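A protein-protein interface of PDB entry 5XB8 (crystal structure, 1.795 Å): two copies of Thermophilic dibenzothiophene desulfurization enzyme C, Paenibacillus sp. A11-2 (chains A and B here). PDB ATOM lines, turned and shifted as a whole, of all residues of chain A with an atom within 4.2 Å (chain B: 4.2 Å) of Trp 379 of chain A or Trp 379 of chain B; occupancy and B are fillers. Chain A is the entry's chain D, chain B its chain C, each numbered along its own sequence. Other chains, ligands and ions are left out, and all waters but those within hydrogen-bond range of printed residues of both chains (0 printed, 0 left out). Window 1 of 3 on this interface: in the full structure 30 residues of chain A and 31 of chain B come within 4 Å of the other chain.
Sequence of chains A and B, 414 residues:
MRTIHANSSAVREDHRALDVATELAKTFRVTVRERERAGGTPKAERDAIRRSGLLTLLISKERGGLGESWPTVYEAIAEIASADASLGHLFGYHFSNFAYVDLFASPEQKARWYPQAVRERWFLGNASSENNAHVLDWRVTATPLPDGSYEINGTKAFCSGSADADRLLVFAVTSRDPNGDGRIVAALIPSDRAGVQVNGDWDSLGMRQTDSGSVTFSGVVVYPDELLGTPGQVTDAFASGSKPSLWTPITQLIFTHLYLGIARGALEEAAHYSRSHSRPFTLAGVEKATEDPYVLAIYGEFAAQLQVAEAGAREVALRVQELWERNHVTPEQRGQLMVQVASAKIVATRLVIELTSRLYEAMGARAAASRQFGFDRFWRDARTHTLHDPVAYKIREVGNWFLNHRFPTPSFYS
Of the 12 printed residues of chain A, 6 touch a printed residue of chain B. Hydrophobic or aromatic side chains of chain A that line the printed part of chain B: Leu 205, Tyr 360 and Trp 379. Of the 12 printed residues of chain B, 6 touch a printed residue of chain A. Among the printed residues, 15 pairs touch across the chains. Among the printed residues, no Asp or Glu carboxylate lies within 4 Å of a Lys or Arg side-chain nitrogen of the other chain.
Ser 357 of chain A touches Trp 379 of chain B, and with the chains exchanged Trp 379 of chain A touches Ser 357 of chain B. Ser 357 of chain A touches Arg 383 of chain B, and with the chains exchanged Arg 383 of chain A touches Ser 357 of chain B. Tyr 360 of chain A touches Trp 379 of chain B, and with the chains exchanged Trp 379 of chain A touches Tyr 360 of chain B. Asp 376 of chain A touches Trp 379 of chain B, and with the chains exchanged Trp 379 of chain A touches Asp 376 of chain B. 12 positions are printed for both chains. Of the 15 pairs that touch across the chains among the printed residues, 15 have their exchanged pair printed and touching as well.
Among the printed residues, pairs that only touch across the chains: Leu 205 of chain A with Tyr 360 of chain B, Leu 205 of chain A with Asp 376 of chain B, Tyr 360 of chain A with Leu 205 of chain B, Tyr 360 of chain A with Trp 379 of chain B, Tyr 360 of chain A with Arg 383 of chain B, Asp 376 of chain A with Leu 205 of chain B, Asp 376 of chain A with Trp 379 of chain B, Trp 379 of chain A with Tyr 360 of chain B, Trp 379 of chain A with Asp 376 of chain B, Trp 379 of chain A with Trp 379 of chain B and Arg 383 of chain A with Tyr 360 of chain B.
Printed residues of chain B within 4 Å of Trp 379 of chain A: Ser 357 (3.0 Å), Tyr 360 (3.98 Å), Asp 376 (3.99 Å) and Trp 379 (3.5 Å). Of chain A, only Ser 357, Tyr 360, Asp 376 and Trp 379 come within 4 Å of Trp 379 of chain B. Of the printed residues of chain A, Asp 376 of chain B touches Leu 205 and Trp 379. Printed residues of chain B within 4 Å of Arg 383 of chain A: Ser 357 and Tyr 360. Printed residues of chain A within 4 Å of Leu 205 of chain B: Tyr 360 (3.7 Å) and Asp 376 (3.3 Å). Arg 377 of chain B touches none of the printed residues of chain A. The nearest printed residue of chain B that does not touch Trp 379 of chain A is Thr 356 of chain B (4.5 Å). The nearest printed residue of chain A that does not touch Trp 379 of chain B is Thr 356 of chain A (4.5 Å).
The side-chain hydroxyl (OG) of Ser 357 of chain B lies within hydrogen-bond range of the indole nitrogen (NE1) of Trp 379 of chain A (3.0 Å). NH1 of Arg 383 of chain B sits at hydrogen-bond distance from O of Ser 357 of chain A, 3.0 Å away. NE1 of Trp 379 of chain B sits at hydrogen-bond distance from OG of Ser 357 of chain A (3.0 Å). O of Ser 357 of chain B lies within hydrogen-bond range of NH1 of Arg 383 of chain A.
The guanidinium group (NE) of Arg 380 of chain A is in salt-bridge range of the side-chain carboxylate (OD2) of Asp 376 of chain A. OD2 of Asp 376 of chain B is in salt-bridge range of NE of Arg 380 of chain B, at 2.8 Å. The side-chain hydroxyl of Tyr 360 of chain B is in hydrogen-bond range of the backbone NH of Asp 376 of chain B, at 3.1 Å. The backbone carbonyl oxygen of Leu 205 of chain A is in hydrogen-bond range of the guanidinium group of Arg 380 of chain A, at 3.0 Å. OH of Tyr 360 of chain A lies within hydrogen-bond range of N of Asp 376 of chain A, 3.1 Å away. The backbone carbonyl oxygen of Leu 205 of chain B sits at hydrogen-bond distance from the guanidinium group of Arg 380 of chain B (2.9 Å).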
ATOM      1  N   LEU A 205       9.031 -14.376 -15.546  1.00  0.00           N
ATOM      2  CA  LEU A 205       9.519 -14.513 -16.920  1.00  0.00           C
ATOM      3  C   LEU A 205      10.823 -15.297 -16.956  1.00  0.00           C
ATOM      4  O   LEU A 205      10.952 -16.300 -17.673  1.00  0.00           O
ATOM      5  CB  LEU A 205       9.715 -13.125 -17.537  1.00  0.00           C
ATOM      6  CG  LEU A 205      10.345 -13.092 -18.918  1.00  0.00           C
ATOM      7  CD1 LEU A 205       9.464 -13.793 -19.944  1.00  0.00           C
ATOM      8  CD2 LEU A 205      10.587 -11.646 -19.300  1.00  0.00           C
ATOM      9  N   THR A 356      21.858 -10.941 -25.457  1.00  0.00           N
ATOM     10  CA  THR A 356      20.964 -12.091 -25.368  1.00  0.00           C
ATOM     11  C   THR A 356      19.853 -12.034 -26.406  1.00  0.00           C
ATOM     12  O   THR A 356      19.304 -13.080 -26.759  1.00  0.00           O
ATOM     13  CB  THR A 356      20.361 -12.234 -23.960  1.00  0.00           C
ATOM     14  OG1 THR A 356      19.644 -11.055 -23.567  1.00  0.00           O
ATOM     15  CG2 THR A 356      21.460 -12.563 -22.935  1.00  0.00           C
ATOM     16  N   SER A 357      19.529 -10.848 -26.915  1.00  0.00           N
ATOM     17  CA  SER A 357      18.564 -10.688 -27.991  1.00  0.00           C
ATOM     18  C   SER A 357      19.226 -10.748 -29.368  1.00  0.00           C
ATOM     19  O   SER A 357      18.766 -11.478 -30.254  1.00  0.00           O
ATOM     20  CB  SER A 357      17.816  -9.359 -27.806  1.00  0.00           C
ATOM     21  OG  SER A 357      16.923  -9.121 -28.876  1.00  0.00           O
ATOM     22  N   TYR A 360      20.689 -13.992 -31.742  1.00  0.00           N
ATOM     23  CA  TYR A 360      19.882 -14.747 -32.701  1.00  0.00           C
ATOM     24  C   TYR A 360      20.263 -14.404 -34.135  1.00  0.00           C
ATOM     25  O   TYR A 360      20.172 -15.253 -35.028  1.00  0.00           O
ATOM     26  CB  TYR A 360      18.395 -14.480 -32.473  1.00  0.00           C
ATOM     27  CG  TYR A 360      17.766 -15.293 -31.367  1.00  0.00           C
ATOM     28  CD1 TYR A 360      17.274 -16.556 -31.621  1.00  0.00           C
ATOM     29  CD2 TYR A 360      17.643 -14.793 -30.073  1.00  0.00           C
ATOM     30  CE1 TYR A 360      16.695 -17.321 -30.615  1.00  0.00           C
ATOM     31  CE2 TYR A 360      17.052 -15.550 -29.069  1.00  0.00           C
ATOM     32  CZ  TYR A 360      16.579 -16.816 -29.355  1.00  0.00           C
ATOM     33  OH  TYR A 360      15.983 -17.590 -28.380  1.00  0.00           O
ATOM     34  N   ASP A 376      16.285 -18.544 -25.468  1.00  0.00           N
ATOM     35  CA  ASP A 376      15.621 -17.351 -24.943  1.00  0.00           C
ATOM     36  C   ASP A 376      15.720 -17.270 -23.426  1.00  0.00           C
ATOM     37  O   ASP A 376      15.436 -16.214 -22.847  1.00  0.00           O
ATOM     38  CB  ASP A 376      14.150 -17.337 -25.371  1.00  0.00           C
ATOM     39  CG  ASP A 376      13.376 -18.530 -24.848  1.00  0.00           C
ATOM     40  OD1 ASP A 376      13.717 -19.671 -25.232  1.00  0.00           O
ATOM     41  OD2 ASP A 376      12.438 -18.331 -24.049  1.00  0.00           O
ATOM     42  N   ARG A 377      16.088 -18.372 -22.772  1.00  0.00           N
ATOM     43  CA  ARG A 377      16.288 -18.361 -21.327  1.00  0.00           C
ATOM     44  C   ARG A 377      17.271 -17.266 -20.910  1.00  0.00           C
ATOM     45  O   ARG A 377      17.080 -16.610 -19.878  1.00  0.00           O
ATOM     46  CB  ARG A 377      16.791 -19.735 -20.882  1.00  0.00           C
ATOM     47  CG  ARG A 377      17.155 -19.839 -19.406  1.00  0.00           C
ATOM     48  CD  ARG A 377      17.478 -21.301 -19.059  1.00  0.00           C
ATOM     49  NE  ARG A 377      18.561 -21.812 -19.901  1.00  0.00           N
ATOM     50  CZ  ARG A 377      19.858 -21.665 -19.643  1.00  0.00           C
ATOM     51  NH1 ARG A 377      20.275 -21.036 -18.547  1.00  0.00           N
ATOM     52  NH2 ARG A 377      20.741 -22.165 -20.478  1.00  0.00           N
ATOM     53  N   PHE A 378      18.332 -17.061 -21.689  1.00  0.00           N
ATOM     54  CA  PHE A 378      19.336 -16.071 -21.309  1.00  0.00           C
ATOM     55  C   PHE A 378      18.718 -14.677 -21.275  1.00  0.00           C
ATOM     56  O   PHE A 378      18.850 -13.952 -20.283  1.00  0.00           O
ATOM     57  CB  PHE A 378      20.537 -16.125 -22.260  1.00  0.00           C
ATOM     58  CG  PHE A 378      21.315 -17.420 -22.206  1.00  0.00           C
ATOM     59  CD1 PHE A 378      22.211 -17.661 -21.186  1.00  0.00           C
ATOM     60  CD2 PHE A 378      21.178 -18.378 -23.207  1.00  0.00           C
ATOM     61  CE1 PHE A 378      22.932 -18.841 -21.133  1.00  0.00           C
ATOM     62  CE2 PHE A 378      21.892 -19.565 -23.158  1.00  0.00           C
ATOM     63  CZ  PHE A 378      22.770 -19.797 -22.128  1.00  0.00           C
ATOM     64  N   TRP A 379      17.983 -14.308 -22.332  1.00  0.00           N
ATOM     65  CA  TRP A 379      17.311 -13.009 -22.335  1.00  0.00           C
ATOM     66  C   TRP A 379      16.264 -12.920 -21.226  1.00  0.00           C
ATOM     67  O   TRP A 379      16.182 -11.911 -20.514  1.00  0.00           O
ATOM     68  CB  TRP A 379      16.677 -12.753 -23.702  1.00  0.00           C
ATOM     69  CG  TRP A 379      15.869 -11.497 -23.721  1.00  0.00           C
ATOM     70  CD1 TRP A 379      16.331 -10.231 -23.929  1.00  0.00           C
ATOM     71  CD2 TRP A 379      14.459 -11.384 -23.510  1.00  0.00           C
ATOM     72  NE1 TRP A 379      15.288  -9.330 -23.867  1.00  0.00           N
ATOM     73  CE2 TRP A 379      14.128 -10.012 -23.618  1.00  0.00           C
ATOM     74  CE3 TRP A 379      13.444 -12.300 -23.248  1.00  0.00           C
ATOM     75  CZ2 TRP A 379      12.827  -9.541 -23.468  1.00  0.00           C
ATOM     76  CZ3 TRP A 379      12.148 -11.831 -23.106  1.00  0.00           C
ATOM     77  CH2 TRP A 379      11.856 -10.455 -23.214  1.00  0.00           C
ATOM     78  N   ARG A 380      15.460 -13.967 -21.048  1.00  0.00           N
ATOM     79  CA  ARG A 380      14.435 -13.918 -20.008  1.00  0.00           C
ATOM     80  C   ARG A 380      15.059 -13.724 -18.626  1.00  0.00           C
ATOM     81  O   ARG A 380      14.574 -12.917 -17.811  1.00  0.00           O
ATOM     82  CB  ARG A 380      13.590 -15.195 -20.039  1.00  0.00           C
ATOM     83  CG  ARG A 380      12.638 -15.281 -21.220  1.00  0.00           C
ATOM     84  CD  ARG A 380      11.655 -16.462 -21.095  1.00  0.00           C
ATOM     85  NE  ARG A 380      12.289 -17.757 -21.342  1.00  0.00           N
ATOM     86  CZ  ARG A 380      12.632 -18.645 -20.412  1.00  0.00           C
ATOM     87  NH1 ARG A 380      12.453 -18.393 -19.120  1.00  0.00           N
ATOM     88  NH2 ARG A 380      13.197 -19.786 -20.777  1.00  0.00           N
ATOM     89  N   ASP A 381      16.146 -14.436 -18.356  1.00  0.00           N
ATOM     90  CA  ASP A 381      16.820 -14.322 -17.068  1.00  0.00           C
ATOM     91  C   ASP A 381      17.402 -12.927 -16.886  1.00  0.00           C
ATOM     92  O   ASP A 381      17.167 -12.264 -15.868  1.00  0.00           O
ATOM     93  CB  ASP A 381      17.929 -15.370 -16.979  1.00  0.00           C
ATOM     94  CG  ASP A 381      17.401 -16.785 -16.795  1.00  0.00           C
ATOM     95  OD1 ASP A 381      16.234 -16.972 -16.372  1.00  0.00           O
ATOM     96  OD2 ASP A 381      18.186 -17.703 -17.051  1.00  0.00           O
ATOM     97  N   ALA A 382      18.145 -12.451 -17.885  1.00  0.00           N
ATOM     98  CA  ALA A 382      18.743 -11.123 -17.789  1.00  0.00           C
ATOM     99  C   ALA A 382      17.673 -10.037 -17.770  1.00  0.00           C
ATOM    100  O   ALA A 382      17.754  -9.078 -16.984  1.00  0.00           O
ATOM    101  CB  ALA A 382      19.698 -10.909 -18.952  1.00  0.00           C
ATOM    102  N   ARG A 383      16.670 -10.154 -18.642  1.00  0.00           N
ATOM    103  CA  ARG A 383      15.636  -9.129 -18.696  1.00  0.00           C
ATOM    104  C   ARG A 383      14.932  -8.992 -17.354  1.00  0.00           C
ATOM    105  O   ARG A 383      14.561  -7.884 -16.958  1.00  0.00           O
ATOM    106  CB  ARG A 383      14.622  -9.442 -19.805  1.00  0.00           C
ATOM    107  CG  ARG A 383      13.528  -8.382 -19.999  1.00  0.00           C
ATOM    108  CD  ARG A 383      14.038  -7.028 -20.472  1.00  0.00           C
ATOM    109  NE  ARG A 383      14.776  -6.303 -19.445  1.00  0.00           N
ATOM    110  CZ  ARG A 383      15.375  -5.125 -19.617  1.00  0.00           C
ATOM    111  NH1 ARG A 383      15.272  -4.460 -20.767  1.00  0.00           N
ATOM    112  NH2 ARG A 383      16.079  -4.595 -18.624  1.00  0.00           N
ATOM    113  N   LEU B 205       9.565 -20.395 -30.668  1.00  0.00           N
ATOM    114  CA  LEU B 205       9.706 -19.386 -29.622  1.00  0.00           C
ATOM    115  C   LEU B 205       8.547 -18.406 -29.668  1.00  0.00           C
ATOM    116  O   LEU B 205       7.859 -18.182 -28.661  1.00  0.00           O
ATOM    117  CB  LEU B 205      11.032 -18.655 -29.800  1.00  0.00           C
ATOM    118  CG  LEU B 205      11.280 -17.448 -28.880  1.00  0.00           C
ATOM    119  CD1 LEU B 205      11.382 -17.895 -27.429  1.00  0.00           C
ATOM    120  CD2 LEU B 205      12.531 -16.736 -29.299  1.00  0.00           C
ATOM    121  N   THR B 356      10.810  -4.069 -28.011  1.00  0.00           N
ATOM    122  CA  THR B 356      10.136  -5.136 -27.271  1.00  0.00           C
ATOM    123  C   THR B 356      10.962  -5.627 -26.079  1.00  0.00           C
ATOM    124  O   THR B 356      10.398  -6.201 -25.138  1.00  0.00           O
ATOM    125  CB  THR B 356       9.782  -6.298 -28.210  1.00  0.00           C
ATOM    126  OG1 THR B 356      10.955  -6.822 -28.826  1.00  0.00           O
ATOM    127  CG2 THR B 356       8.781  -5.856 -29.276  1.00  0.00           C
ATOM    128  N   SER B 357      12.271  -5.386 -26.082  1.00  0.00           N
ATOM    129  CA  SER B 357      13.119  -5.708 -24.944  1.00  0.00           C
ATOM    130  C   SER B 357      13.245  -4.525 -23.981  1.00  0.00           C
ATOM    131  O   SER B 357      13.073  -4.673 -22.766  1.00  0.00           O
ATOM    132  CB  SER B 357      14.498  -6.146 -25.452  1.00  0.00           C
ATOM    133  OG  SER B 357      15.402  -6.386 -24.382  1.00  0.00           O
ATOM    134  N   TYR B 360      10.656  -2.945 -21.013  1.00  0.00           N
ATOM    135  CA  TYR B 360      10.615  -3.405 -19.626  1.00  0.00           C
ATOM    136  C   TYR B 360      11.237  -2.383 -18.689  1.00  0.00           C
ATOM    137  O   TYR B 360      10.790  -2.232 -17.549  1.00  0.00           O
ATOM    138  CB  TYR B 360      11.345  -4.741 -19.484  1.00  0.00           C
ATOM    139  CG  TYR B 360      10.511  -5.936 -19.834  1.00  0.00           C
ATOM    140  CD1 TYR B 360       9.691  -6.520 -18.900  1.00  0.00           C
ATOM    141  CD2 TYR B 360      10.540  -6.477 -21.106  1.00  0.00           C
ATOM    142  CE1 TYR B 360       8.922  -7.620 -19.208  1.00  0.00           C
ATOM    143  CE2 TYR B 360       9.780  -7.567 -21.427  1.00  0.00           C
ATOM    144  CZ  TYR B 360       8.969  -8.141 -20.476  1.00  0.00           C
ATOM    145  OH  TYR B 360       8.202  -9.237 -20.795  1.00  0.00           O
ATOM    146  N   ASP B 376       6.344 -10.528 -22.900  1.00  0.00           N
ATOM    147  CA  ASP B 376       7.451 -11.070 -23.673  1.00  0.00           C
ATOM    148  C   ASP B 376       6.999 -11.684 -24.991  1.00  0.00           C
ATOM    149  O   ASP B 376       7.847 -11.978 -25.839  1.00  0.00           O
ATOM    150  CB  ASP B 376       8.182 -12.124 -22.848  1.00  0.00           C
ATOM    151  CG  ASP B 376       7.291 -13.284 -22.501  1.00  0.00           C
ATOM    152  OD1 ASP B 376       6.277 -13.065 -21.797  1.00  0.00           O
ATOM    153  OD2 ASP B 376       7.610 -14.402 -22.944  1.00  0.00           O
ATOM    154  N   ARG B 377       5.695 -11.894 -25.160  1.00  0.00           N
ATOM    155  CA  ARG B 377       5.163 -12.372 -26.432  1.00  0.00           C
ATOM    156  C   ARG B 377       5.589 -11.470 -27.579  1.00  0.00           C
ATOM    157  O   ARG B 377       5.906 -11.958 -28.667  1.00  0.00           O
ATOM    158  CB  ARG B 377       3.633 -12.455 -26.352  1.00  0.00           C
ATOM    159  CG  ARG B 377       2.950 -12.814 -27.678  1.00  0.00           C
ATOM    160  CD  ARG B 377       1.447 -12.970 -27.474  1.00  0.00           C
ATOM    161  NE  ARG B 377       0.844 -11.778 -26.880  1.00  0.00           N
ATOM    162  CZ  ARG B 377       0.379 -10.735 -27.559  1.00  0.00           C
ATOM    163  NH1 ARG B 377       0.407 -10.703 -28.892  1.00  0.00           N
ATOM    164  NH2 ARG B 377      -0.119  -9.710 -26.892  1.00  0.00           N
ATOM    165  N   PHE B 378       5.596 -10.150 -27.370  1.00  0.00           N
ATOM    166  CA  PHE B 378       5.975  -9.251 -28.460  1.00  0.00           C
ATOM    167  C   PHE B 378       7.424  -9.484 -28.889  1.00  0.00           C
ATOM    168  O   PHE B 378       7.715  -9.592 -30.092  1.00  0.00           O
ATOM    169  CB  PHE B 378       5.766  -7.788 -28.059  1.00  0.00           C
ATOM    170  CG  PHE B 378       4.333  -7.426 -27.775  1.00  0.00           C
ATOM    171  CD1 PHE B 378       3.451  -7.138 -28.812  1.00  0.00           C
ATOM    172  CD2 PHE B 378       3.870  -7.340 -26.480  1.00  0.00           C
ATOM    173  CE1 PHE B 378       2.158  -6.800 -28.556  1.00  0.00           C
ATOM    174  CE2 PHE B 378       2.559  -7.000 -26.221  1.00  0.00           C
ATOM    175  CZ  PHE B 378       1.702  -6.726 -27.267  1.00  0.00           C
ATOM    176  N   TRP B 379       8.352  -9.564 -27.921  1.00  0.00           N
ATOM    177  CA  TRP B 379       9.743  -9.857 -28.258  1.00  0.00           C
ATOM    178  C   TRP B 379       9.871 -11.235 -28.885  1.00  0.00           C
ATOM    179  O   TRP B 379      10.558 -11.404 -29.897  1.00  0.00           O
ATOM    180  CB  TRP B 379      10.649  -9.746 -27.025  1.00  0.00           C
ATOM    181  CG  TRP B 379      12.058 -10.159 -27.306  1.00  0.00           C
ATOM    182  CD1 TRP B 379      13.049  -9.388 -27.840  1.00  0.00           C
ATOM    183  CD2 TRP B 379      12.639 -11.453 -27.081  1.00  0.00           C
ATOM    184  NE1 TRP B 379      14.208 -10.122 -27.977  1.00  0.00           N
ATOM    185  CE2 TRP B 379      13.984 -11.387 -27.506  1.00  0.00           C
ATOM    186  CE3 TRP B 379      12.153 -12.654 -26.558  1.00  0.00           C
ATOM    187  CZ2 TRP B 379      14.853 -12.474 -27.415  1.00  0.00           C
ATOM    188  CZ3 TRP B 379      13.015 -13.739 -26.478  1.00  0.00           C
ATOM    189  CH2 TRP B 379      14.351 -13.640 -26.906  1.00  0.00           C
ATOM    190  N   ARG B 380       9.206 -12.236 -28.315  1.00  0.00           N
ATOM    191  CA  ARG B 380       9.323 -13.572 -28.877  1.00  0.00           C
ATOM    192  C   ARG B 380       8.831 -13.604 -30.322  1.00  0.00           C
ATOM    193  O   ARG B 380       9.468 -14.225 -31.175  1.00  0.00           O
ATOM    194  CB  ARG B 380       8.553 -14.586 -28.031  1.00  0.00           C
ATOM    195  CG  ARG B 380       9.212 -14.889 -26.685  1.00  0.00           C
ATOM    196  CD  ARG B 380       8.547 -16.067 -25.961  1.00  0.00           C
ATOM    197  NE  ARG B 380       7.259 -15.705 -25.373  1.00  0.00           N
ATOM    198  CZ  ARG B 380       6.071 -15.992 -25.897  1.00  0.00           C
ATOM    199  NH1 ARG B 380       5.961 -16.664 -27.037  1.00  0.00           N
ATOM    200  NH2 ARG B 380       4.982 -15.627 -25.268  1.00  0.00           N
ATOM    201  N   ASP B 381       7.688 -12.970 -30.601  1.00  0.00           N
ATOM    202  CA  ASP B 381       7.152 -12.948 -31.967  1.00  0.00           C
ATOM    203  C   ASP B 381       8.100 -12.228 -32.916  1.00  0.00           C
ATOM    204  O   ASP B 381       8.416 -12.726 -34.004  1.00  0.00           O
ATOM    205  CB  ASP B 381       5.783 -12.261 -31.985  1.00  0.00           C
ATOM    206  CG  ASP B 381       4.693 -13.072 -31.304  1.00  0.00           C
ATOM    207  OD1 ASP B 381       4.841 -14.312 -31.163  1.00  0.00           O
ATOM    208  OD2 ASP B 381       3.680 -12.452 -30.922  1.00  0.00           O
ATOM    209  N   ALA B 382       8.529 -11.028 -32.531  1.00  0.00           N
ATOM    210  CA  ALA B 382       9.420 -10.236 -33.373  1.00  0.00           C
ATOM    211  C   ALA B 382      10.774 -10.913 -33.541  1.00  0.00           C
ATOM    212  O   ALA B 382      11.312 -10.963 -34.652  1.00  0.00           O
ATOM    213  CB  ALA B 382       9.591  -8.837 -32.781  1.00  0.00           C
ATOM    214  N   ARG B 383      11.336 -11.454 -32.454  1.00  0.00           N
ATOM    215  CA  ARG B 383      12.641 -12.095 -32.547  1.00  0.00           C
ATOM    216  C   ARG B 383      12.587 -13.297 -33.480  1.00  0.00           C
ATOM    217  O   ARG B 383      13.542 -13.567 -34.212  1.00  0.00           O
ATOM    218  CB  ARG B 383      13.131 -12.520 -31.153  1.00  0.00           C
ATOM    219  CG  ARG B 383      14.523 -13.188 -31.132  1.00  0.00           C
ATOM    220  CD  ARG B 383      15.652 -12.235 -31.491  1.00  0.00           C
ATOM    221  NE  ARG B 383      15.660 -11.884 -32.909  1.00  0.00           N
ATOM    222  CZ  ARG B 383      16.519 -11.040 -33.477  1.00  0.00           C
ATOM    223  NH1 ARG B 383      17.510 -10.489 -32.778  1.00  0.00           N
ATOM    224  NH2 ARG B 383      16.395 -10.761 -34.758  1.00  0.00           N
